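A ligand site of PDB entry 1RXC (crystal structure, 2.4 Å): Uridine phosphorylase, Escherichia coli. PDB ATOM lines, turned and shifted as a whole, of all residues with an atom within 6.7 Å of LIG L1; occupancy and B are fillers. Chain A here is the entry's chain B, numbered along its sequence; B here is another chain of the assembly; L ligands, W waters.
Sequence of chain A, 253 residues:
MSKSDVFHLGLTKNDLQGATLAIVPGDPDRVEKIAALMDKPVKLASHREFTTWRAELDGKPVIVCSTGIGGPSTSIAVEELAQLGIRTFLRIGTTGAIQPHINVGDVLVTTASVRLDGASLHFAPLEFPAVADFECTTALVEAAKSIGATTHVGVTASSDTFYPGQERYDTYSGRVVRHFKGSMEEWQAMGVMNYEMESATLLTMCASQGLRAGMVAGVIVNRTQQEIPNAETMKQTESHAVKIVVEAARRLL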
ATOM      1  N   ARG A  91      27.406   2.754 -19.077  1.00  0.00           N
ATOM      2  CA  ARG A  91      26.712   3.595 -20.046  1.00  0.00           C
ATOM      3  C   ARG A  91      27.479   3.642 -21.360  1.00  0.00           C
ATOM      4  O   ARG A  91      28.690   3.813 -21.372  1.00  0.00           O
ATOM      5  CB  ARG A  91      26.500   5.004 -19.511  1.00  0.00           C
ATOM      6  CG  ARG A  91      25.769   5.889 -20.515  1.00  0.00           C
ATOM      7  CD  ARG A  91      25.306   7.203 -19.952  1.00  0.00           C
ATOM      8  NE  ARG A  91      25.430   8.292 -20.916  1.00  0.00           N
ATOM      9  CZ  ARG A  91      24.703   8.405 -22.022  1.00  0.00           C
ATOM     10  NH1 ARG A  91      23.775   7.502 -22.326  1.00  0.00           N
ATOM     11  NH2 ARG A  91      24.911   9.441 -22.835  1.00  0.00           N
ATOM     12  N   THR A  94      26.072   8.799 -26.887  1.00  0.00           N
ATOM     13  CA  THR A  94      26.552   9.669 -27.956  1.00  0.00           C
ATOM     14  C   THR A  94      26.888  11.007 -27.336  1.00  0.00           C
ATOM     15  O   THR A  94      26.328  11.388 -26.326  1.00  0.00           O
ATOM     16  CB  THR A  94      25.489   9.859 -29.064  1.00  0.00           C
ATOM     17  OG1 THR A  94      24.308  10.480 -28.522  1.00  0.00           O
ATOM     18  CG2 THR A  94      25.027   8.497 -29.602  1.00  0.00           C
ATOM     19  N   THR A  95      27.813  11.740 -27.946  1.00  0.00           N
ATOM     20  CA  THR A  95      28.321  12.941 -27.310  1.00  0.00           C
ATOM     21  C   THR A  95      28.833  13.960 -28.314  1.00  0.00           C
ATOM     22  O   THR A  95      29.149  13.621 -29.450  1.00  0.00           O
ATOM     23  CB  THR A  95      29.405  12.542 -26.265  1.00  0.00           C
ATOM     24  OG1 THR A  95      29.731  13.657 -25.433  1.00  0.00           O
ATOM     25  CG2 THR A  95      30.711  12.150 -26.914  1.00  0.00           C
ATOM     26  N   GLY A  96      28.864  15.231 -27.907  1.00  0.00           N
ATOM     27  CA  GLY A  96      29.501  16.286 -28.668  1.00  0.00           C
ATOM     28  C   GLY A  96      30.819  16.664 -28.008  1.00  0.00           C
ATOM     29  O   GLY A  96      30.840  17.020 -26.854  1.00  0.00           O
ATOM     30  N   ALA A  97      31.919  16.556 -28.748  1.00  0.00           N
ATOM     31  CA  ALA A  97      33.218  17.006 -28.293  1.00  0.00           C
ATOM     32  C   ALA A  97      33.327  18.527 -28.350  1.00  0.00           C
ATOM     33  O   ALA A  97      32.755  19.170 -29.233  1.00  0.00           O
ATOM     34  CB  ALA A  97      34.310  16.366 -29.137  1.00  0.00           C
ATOM     35  N   SER A 159      25.038  17.497 -18.581  1.00  0.00           N
ATOM     36  CA  SER A 159      24.085  18.606 -18.532  1.00  0.00           C
ATOM     37  C   SER A 159      22.637  18.135 -18.570  1.00  0.00           C
ATOM     38  O   SER A 159      22.288  17.243 -19.334  1.00  0.00           O
ATOM     39  CB  SER A 159      24.374  19.518 -19.725  1.00  0.00           C
ATOM     40  OG  SER A 159      23.448  20.566 -19.891  1.00  0.00           O
ATOM     41  N   THR A 161      20.277  19.812 -19.774  1.00  0.00           N
ATOM     42  CA  THR A 161      19.713  20.199 -21.079  1.00  0.00           C
ATOM     43  C   THR A 161      20.623  19.840 -22.240  1.00  0.00           C
ATOM     44  O   THR A 161      21.824  19.618 -22.075  1.00  0.00           O
ATOM     45  CB  THR A 161      19.410  21.696 -21.146  1.00  0.00           C
ATOM     46  OG1 THR A 161      20.584  22.445 -20.785  1.00  0.00           O
ATOM     47  CG2 THR A 161      18.313  22.114 -20.135  1.00  0.00           C
ATOM     48  N   PHE A 162      20.006  19.781 -23.411  1.00  0.00           N
ATOM     49  CA  PHE A 162      20.722  19.644 -24.671  1.00  0.00           C
ATOM     50  C   PHE A 162      21.081  21.019 -25.212  1.00  0.00           C
ATOM     51  O   PHE A 162      22.117  21.183 -25.848  1.00  0.00           O
ATOM     52  CB  PHE A 162      19.865  18.889 -25.699  1.00  0.00           C
ATOM     53  CG  PHE A 162      20.617  18.525 -26.940  1.00  0.00           C
ATOM     54  CD1 PHE A 162      21.558  17.485 -26.930  1.00  0.00           C
ATOM     55  CD2 PHE A 162      20.414  19.236 -28.125  1.00  0.00           C
ATOM     56  CE1 PHE A 162      22.255  17.163 -28.074  1.00  0.00           C
ATOM     57  CE2 PHE A 162      21.111  18.914 -29.269  1.00  0.00           C
ATOM     58  CZ  PHE A 162      22.030  17.867 -29.249  1.00  0.00           C
ATOM     59  N   GLN A 166      24.514  23.281 -22.799  1.00  0.00           N
ATOM     60  CA  GLN A 166      25.601  22.959 -23.692  1.00  0.00           C
ATOM     61  C   GLN A 166      25.918  24.166 -24.584  1.00  0.00           C
ATOM     62  O   GLN A 166      26.608  24.062 -25.595  1.00  0.00           O
ATOM     63  CB  GLN A 166      25.254  21.704 -24.498  1.00  0.00           C
ATOM     64  CG  GLN A 166      24.941  20.520 -23.583  1.00  0.00           C
ATOM     65  CD  GLN A 166      24.796  19.201 -24.303  1.00  0.00           C
ATOM     66  OE1 GLN A 166      25.417  18.984 -25.370  1.00  0.00           O
ATOM     67  NE2 GLN A 166      23.996  18.301 -23.724  1.00  0.00           N
ATOM     68  N   ARG A 168      24.161  26.061 -26.697  1.00  0.00           N
ATOM     69  CA  ARG A 168      23.651  26.141 -28.054  1.00  0.00           C
ATOM     70  C   ARG A 168      22.790  27.381 -28.109  1.00  0.00           C
ATOM     71  O   ARG A 168      21.999  27.630 -27.195  1.00  0.00           O
ATOM     72  CB  ARG A 168      22.814  24.915 -28.387  1.00  0.00           C
ATOM     73  CG  ARG A 168      23.621  23.747 -28.911  1.00  0.00           C
ATOM     74  CD  ARG A 168      22.806  22.486 -29.129  1.00  0.00           C
ATOM     75  NE  ARG A 168      23.624  21.439 -29.740  1.00  0.00           N
ATOM     76  CZ  ARG A 168      24.236  20.453 -29.074  1.00  0.00           C
ATOM     77  NH1 ARG A 168      24.127  20.326 -27.755  1.00  0.00           N
ATOM     78  NH2 ARG A 168      24.966  19.570 -29.744  1.00  0.00           N
ATOM     79  N   TYR A 195      30.325  17.040 -24.071  1.00  0.00           N
ATOM     80  CA  TYR A 195      29.059  17.155 -23.362  1.00  0.00           C
ATOM     81  C   TYR A 195      28.239  15.899 -23.616  1.00  0.00           C
ATOM     82  O   TYR A 195      28.166  15.399 -24.748  1.00  0.00           O
ATOM     83  CB  TYR A 195      28.235  18.297 -23.914  1.00  0.00           C
ATOM     84  CG  TYR A 195      28.599  19.714 -23.497  1.00  0.00           C
ATOM     85  CD1 TYR A 195      28.385  20.158 -22.196  1.00  0.00           C
ATOM     86  CD2 TYR A 195      29.067  20.619 -24.427  1.00  0.00           C
ATOM     87  CE1 TYR A 195      28.678  21.473 -21.844  1.00  0.00           C
ATOM     88  CE2 TYR A 195      29.352  21.907 -24.090  1.00  0.00           C
ATOM     89  CZ  TYR A 195      29.164  22.334 -22.795  1.00  0.00           C
ATOM     90  OH  TYR A 195      29.465  23.637 -22.492  1.00  0.00           O
ATOM     91  N   GLU A 196      27.603  15.409 -22.562  1.00  0.00           N
ATOM     92  CA  GLU A 196      26.449  14.533 -22.693  1.00  0.00           C
ATOM     93  C   GLU A 196      25.499  14.805 -21.516  1.00  0.00           C
ATOM     94  O   GLU A 196      25.614  15.852 -20.898  1.00  0.00           O
ATOM     95  CB  GLU A 196      26.891  13.072 -22.828  1.00  0.00           C
ATOM     96  CG  GLU A 196      27.784  12.576 -21.715  1.00  0.00           C
ATOM     97  CD  GLU A 196      26.970  12.193 -20.503  1.00  0.00           C
ATOM     98  OE1 GLU A 196      26.217  11.225 -20.618  1.00  0.00           O
ATOM     99  OE2 GLU A 196      27.046  12.908 -19.471  1.00  0.00           O
ATOM    100  N   MET A 197      24.558  13.923 -21.212  1.00  0.00           N
ATOM    101  CA  MET A 197      23.433  14.276 -20.337  1.00  0.00           C
ATOM    102  C   MET A 197      23.152  13.327 -19.143  1.00  0.00           C
ATOM    103  O   MET A 197      22.457  13.729 -18.214  1.00  0.00           O
ATOM    104  CB  MET A 197      22.164  14.451 -21.184  1.00  0.00           C
ATOM    105  CG  MET A 197      22.262  15.580 -22.191  1.00  0.00           C
ATOM    106  SD  MET A 197      20.755  15.946 -23.113  1.00  0.00           S
ATOM    107  CE  MET A 197      19.767  16.697 -21.852  1.00  0.00           C
ATOM    108  N   GLU A 198      23.692  12.114 -19.139  1.00  0.00           N
ATOM    109  CA  GLU A 198      23.356  11.131 -18.094  1.00  0.00           C
ATOM    110  C   GLU A 198      24.467  10.767 -17.117  1.00  0.00           C
ATOM    111  O   GLU A 198      24.192  10.307 -16.028  1.00  0.00           O
ATOM    112  CB  GLU A 198      22.848   9.840 -18.731  1.00  0.00           C
ATOM    113  CG  GLU A 198      21.529   9.991 -19.459  1.00  0.00           C
ATOM    114  CD  GLU A 198      21.693  10.605 -20.836  1.00  0.00           C
ATOM    115  OE1 GLU A 198      22.736  10.342 -21.477  1.00  0.00           O
ATOM    116  OE2 GLU A 198      20.799  11.358 -21.250  1.00  0.00           O
ATOM    117  N   GLY A 218      30.356   7.810 -28.101  1.00  0.00           N
ATOM    118  CA  GLY A 218      30.860   8.028 -29.439  1.00  0.00           C
ATOM    119  C   GLY A 218      30.583   9.464 -29.851  1.00  0.00           C
ATOM    120  O   GLY A 218      29.499   9.976 -29.590  1.00  0.00           O
ATOM    121  N   VAL A 219      31.562  10.091 -30.478  1.00  0.00           N
ATOM    122  CA  VAL A 219      31.501  11.506 -30.816  1.00  0.00           C
ATOM    123  C   VAL A 219      30.734  11.622 -32.130  1.00  0.00           C
ATOM    124  O   VAL A 219      31.157  11.085 -33.165  1.00  0.00           O
ATOM    125  CB  VAL A 219      32.932  12.113 -30.969  1.00  0.00           C
ATOM    126  CG1 VAL A 219      32.872  13.582 -31.356  1.00  0.00           C
ATOM    127  CG2 VAL A 219      33.709  11.977 -29.659  1.00  0.00           C
ATOM    128  N   ILE A 220      29.600  12.304 -32.086  1.00  0.00           N
ATOM    129  CA  ILE A 220      28.802  12.505 -33.285  1.00  0.00           C
ATOM    130  C   ILE A 220      28.853  13.953 -33.757  1.00  0.00           C
ATOM    131  O   ILE A 220      28.329  14.265 -34.824  1.00  0.00           O
ATOM    132  CB  ILE A 220      27.345  12.028 -33.080  1.00  0.00           C
ATOM    133  CG1 ILE A 220      26.704  12.706 -31.869  1.00  0.00           C
ATOM    134  CG2 ILE A 220      27.307  10.525 -32.910  1.00  0.00           C
ATOM    135  CD1 ILE A 220      25.210  12.692 -31.919  1.00  0.00           C
ATOM    136  N   VAL A 221      29.465  14.825 -32.968  1.00  0.00           N
ATOM    137  CA  VAL A 221      29.647  16.215 -33.387  1.00  0.00           C
ATOM    138  C   VAL A 221      30.766  16.867 -32.606  1.00  0.00           C
ATOM    139  O   VAL A 221      31.007  16.506 -31.460  1.00  0.00           O
ATOM    140  CB  VAL A 221      28.342  17.051 -33.232  1.00  0.00           C
ATOM    141  CG1 VAL A 221      28.064  17.416 -31.770  1.00  0.00           C
ATOM    142  CG2 VAL A 221      28.427  18.321 -34.081  1.00  0.00           C
ATOM    143  N   ARG A 223      31.794  20.653 -31.387  1.00  0.00           N
ATOM    144  CA  ARG A 223      31.180  21.952 -31.142  1.00  0.00           C
ATOM    145  C   ARG A 223      32.028  23.179 -31.574  1.00  0.00           C
ATOM    146  O   ARG A 223      31.551  24.302 -31.548  1.00  0.00           O
ATOM    147  CB  ARG A 223      30.789  22.059 -29.663  1.00  0.00           C
ATOM    148  CG  ARG A 223      29.735  20.992 -29.242  1.00  0.00           C
ATOM    149  CD  ARG A 223      28.421  21.169 -29.932  1.00  0.00           C
ATOM    150  NE  ARG A 223      28.050  22.563 -29.766  1.00  0.00           N
ATOM    151  CZ  ARG A 223      27.496  23.082 -28.672  1.00  0.00           C
ATOM    152  NH1 ARG A 223      27.260  24.385 -28.621  1.00  0.00           N
ATOM    153  NH2 ARG A 223      27.153  22.297 -27.656  1.00  0.00           N
ATOM    154  N   GLU A 227      26.752  23.248 -34.111  1.00  0.00           N
ATOM    155  CA  GLU A 227      25.866  22.924 -32.993  1.00  0.00           C
ATOM    156  C   GLU A 227      25.205  21.545 -33.124  1.00  0.00           C
ATOM    157  O   GLU A 227      25.205  20.771 -32.184  1.00  0.00           O
ATOM    158  CB  GLU A 227      24.814  24.000 -32.805  1.00  0.00           C
ATOM    159  CG  GLU A 227      25.387  25.279 -32.236  1.00  0.00           C
ATOM    160  CD  GLU A 227      24.333  26.223 -31.676  1.00  0.00           C
ATOM    161  OE1 GLU A 227      23.149  25.820 -31.496  1.00  0.00           O
ATOM    162  OE2 GLU A 227      24.687  27.383 -31.417  1.00  0.00           O
ATOM    163  N   PRO A 229      24.535  17.747 -34.837  1.00  0.00           N
ATOM    164  CA  PRO A 229      25.219  16.658 -35.543  1.00  0.00           C
ATOM    165  C   PRO A 229      24.702  16.379 -36.956  1.00  0.00           C
ATOM    166  O   PRO A 229      23.518  16.546 -37.220  1.00  0.00           O
ATOM    167  CB  PRO A 229      24.959  15.441 -34.640  1.00  0.00           C
ATOM    168  CG  PRO A 229      24.660  16.007 -33.295  1.00  0.00           C
ATOM    169  CD  PRO A 229      23.934  17.277 -33.580  1.00  0.00           C
ATOM    170  N   PHE B   7      16.284  18.057 -34.305  1.00  0.00           N
ATOM    171  CA  PHE B   7      17.227  16.949 -34.156  1.00  0.00           C
ATOM    172  C   PHE B   7      16.632  15.685 -33.519  1.00  0.00           C
ATOM    173  O   PHE B   7      16.907  14.582 -33.968  1.00  0.00           O
ATOM    174  CB  PHE B   7      18.481  17.401 -33.414  1.00  0.00           C
ATOM    175  CG  PHE B   7      19.542  16.365 -33.379  1.00  0.00           C
ATOM    176  CD1 PHE B   7      20.125  15.910 -34.563  1.00  0.00           C
ATOM    177  CD2 PHE B   7      19.952  15.793 -32.178  1.00  0.00           C
ATOM    178  CE1 PHE B   7      21.085  14.923 -34.545  1.00  0.00           C
ATOM    179  CE2 PHE B   7      20.925  14.807 -32.154  1.00  0.00           C
ATOM    180  CZ  PHE B   7      21.481  14.368 -33.332  1.00  0.00           C
ATOM    181  N   HIS B   8      15.844  15.835 -32.466  1.00  0.00           N
ATOM    182  CA  HIS B   8      15.341  14.676 -31.693  1.00  0.00           C
ATOM    183  C   HIS B   8      13.943  14.152 -32.108  1.00  0.00           C
ATOM    184  O   HIS B   8      13.755  12.940 -32.224  1.00  0.00           O
ATOM    185  CB  HIS B   8      15.325  15.007 -30.188  1.00  0.00           C
ATOM    186  CG  HIS B   8      16.691  15.189 -29.598  1.00  0.00           C
ATOM    187  ND1 HIS B   8      17.319  16.415 -29.545  1.00  0.00           N
ATOM    188  CD2 HIS B   8      17.539  14.304 -29.011  1.00  0.00           C
ATOM    189  CE1 HIS B   8      18.492  16.280 -28.953  1.00  0.00           C
ATOM    190  NE2 HIS B   8      18.653  15.019 -28.622  1.00  0.00           N
HETATM  191  N1  LIG L   1      24.438  14.226 -26.881  1.00  0.00           N
HETATM  192  C1  LIG L   1      24.620  15.372 -26.190  1.00  0.00           C
HETATM  193  N2  LIG L   1      25.293  16.407 -26.716  1.00  0.00           N
HETATM  194  C2  LIG L   1      25.822  16.336 -27.947  1.00  0.00           C
HETATM  195  C3  LIG L   1      25.626  15.077 -28.691  1.00  0.00           C
HETATM  196  C4  LIG L   1      24.919  14.041 -28.111  1.00  0.00           C
HETATM  197  O1  LIG L   1      24.137  15.481 -25.052  1.00  0.00           O
HETATM  198  O2  LIG L   1      26.456  17.288 -28.443  1.00  0.00           O
HETATM  199  F1  LIG L   1      26.117  14.966 -29.909  1.00  0.00           F
HETATM  200  C1  LG2 L   2      20.899  13.681 -26.503  1.00  0.00           C
HETATM  201  O1  LG2 L   2      20.962  13.656 -27.907  1.00  0.00           O
HETATM  202  C2  LG2 L   2      21.264  12.380 -25.802  1.00  0.00           C
HETATM  203  O2  LG2 L   2      22.558  12.055 -26.298  1.00  0.00           O
HETATM  204  C3  LG2 L   2      23.360  11.259 -25.437  1.00  0.00           C
HETATM  205  C4  LG2 L   2      23.014  12.225 -24.295  1.00  0.00           C
HETATM  206  O3  LG2 L   2      23.678  12.000 -23.064  1.00  0.00           O
HETATM  207  C5  LG2 L   2      21.493  12.308 -24.306  1.00  0.00           C
HETATM  208  O4  LG2 L   2      20.803  11.151 -23.874  1.00  0.00           O
HETATM  209  O5  LG2 L   2      23.454   9.831 -25.360  1.00  0.00           O
HETATM  210  P1  LG2 L   2      22.479   8.669 -25.878  1.00  0.00           P
HETATM  211  O6  LG2 L   2      21.106   9.138 -25.444  1.00  0.00           O
HETATM  212  O7  LG2 L   2      22.964   7.464 -25.114  1.00  0.00           O
HETATM  213  O8  LG2 L   2      22.673   8.611 -27.373  1.00  0.00           O
HETATM  214  O   HOH W   1      27.371  19.499 -27.192  1.00  0.00           O
HETATM  215  O   HOH W   2      22.443  12.316 -29.833  1.00  0.00           O
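The side-chain amide oxygen (OE1) of Gln 166 sits at hydrogen-bond distance from a nitrogen (N2) of LIG L1 (2.9 Å).
An oxygen (O2) of LIG L1 is in hydrogen-bond range of the guanidinium group (NH2) of Arg 168 (3.0 Å).
An oxygen (O2) of LIG L1 sits at hydrogen-bond distance from the backbone NH of Gly 96 (3.2 Å).
The backbone carbonyl oxygen (O) of Thr 94 lies within hydrogen-bond range of a nitrogen (N1) of LIG L1 (3.5 Å).
O3 of LG2 L2 lies within hydrogen-bond range of N of Met 197, 2.8 Å away.
The backbone NH (N) of Thr 94 sits at hydrogen-bond distance from an oxygen (O5) of LG2 L2 (3.2 Å).
The side-chain hydroxyl (OG1) of Thr 94 sits at hydrogen-bond distance from an oxygen (O8) of LG2 L2.
NE2 of His 8 of chain B is in hydrogen-bond range of O1 of LG2 L2 (2.8 Å).
The guanidinium group of Arg 91 is in salt-bridge range of an oxygen (O7) of LG2 L2, at 2.9 Å.
An oxygen (O3) of LG2 L2 is in hydrogen-bond range of the side-chain carboxylate (OE1) of Glu 198, 2.5 Å away.
O2 of LG2 L2 lies within hydrogen-bond range of N1 of LIG L1.
The side-chain amide nitrogen of Gln 166 lies within hydrogen-bond range of the backbone carbonyl oxygen of Thr 161.
The guanidinium group (NH1) of Arg 168 lies within hydrogen-bond range of the backbone carbonyl oxygen (O) of Phe 162 (2.9 Å).
The backbone carbonyl oxygen of Gly 96 sits at hydrogen-bond distance from the backbone NH of Tyr 195 (2.8 Å).
O of Tyr 195 is in hydrogen-bond range of OG1 of Thr 95, at 2.4 Å.
The backbone NH (N) of Thr 95 lies within hydrogen-bond range of the backbone carbonyl oxygen (O) of Gly 218.
The side-chain carboxylate (OE1) of Glu 196 is in salt-bridge range of the guanidinium group (NE) of Arg 91 (3.1 Å).
N of Glu 198 lies within hydrogen-bond range of OE1 of Glu 196, 3.1 Å away.
O of Val 221 lies within hydrogen-bond range of N of Ala 97 (2.9 Å).
The backbone carbonyl oxygen (O) of Thr 95 lies close to a fluorine (F1) of LIG L1, 3.3 Å away.
Merely in contact with LIG L1: Phe 162 (3.4 Å), Tyr 195 (3.6 Å), Glu 196 (3.4 Å), Met 197 (3.4 Å), Ile 220 (3.0 Å), Val 221 (3.6 Å) and Pro 229 (3.8 Å).
Hydrophobic or aromatic side chains within 4 Å of LIG L1: Phe 162, Met 197, Ile 220, Val 221 and Pro 229.
Within 4 Å of LIG L1: Thr 94, Thr 95, Gly 96, Phe 162, Gln 166, Arg 168, Tyr 195, Glu 196, Met 197, Ile 220, Val 221 and Pro 229.
The nearest printed residue that does not touch LIG L1 is Arg 223 (4.6 Å).
Water W1 lies within hydrogen-bond range of an oxygen (O2) of LIG L1 (2.7 Å), the side-chain amide oxygen (OE1) of Gln 166 (2.7 Å), the guanidinium group (NH2) of Arg 223 (2.8 Å) and the guanidinium group (NH1) of Arg 168 (3.4 Å).
Water W2 lies within hydrogen-bond range of O1 of LG2 L2 (2.8 Å) and OG1 of Thr 94 (2.9 Å).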
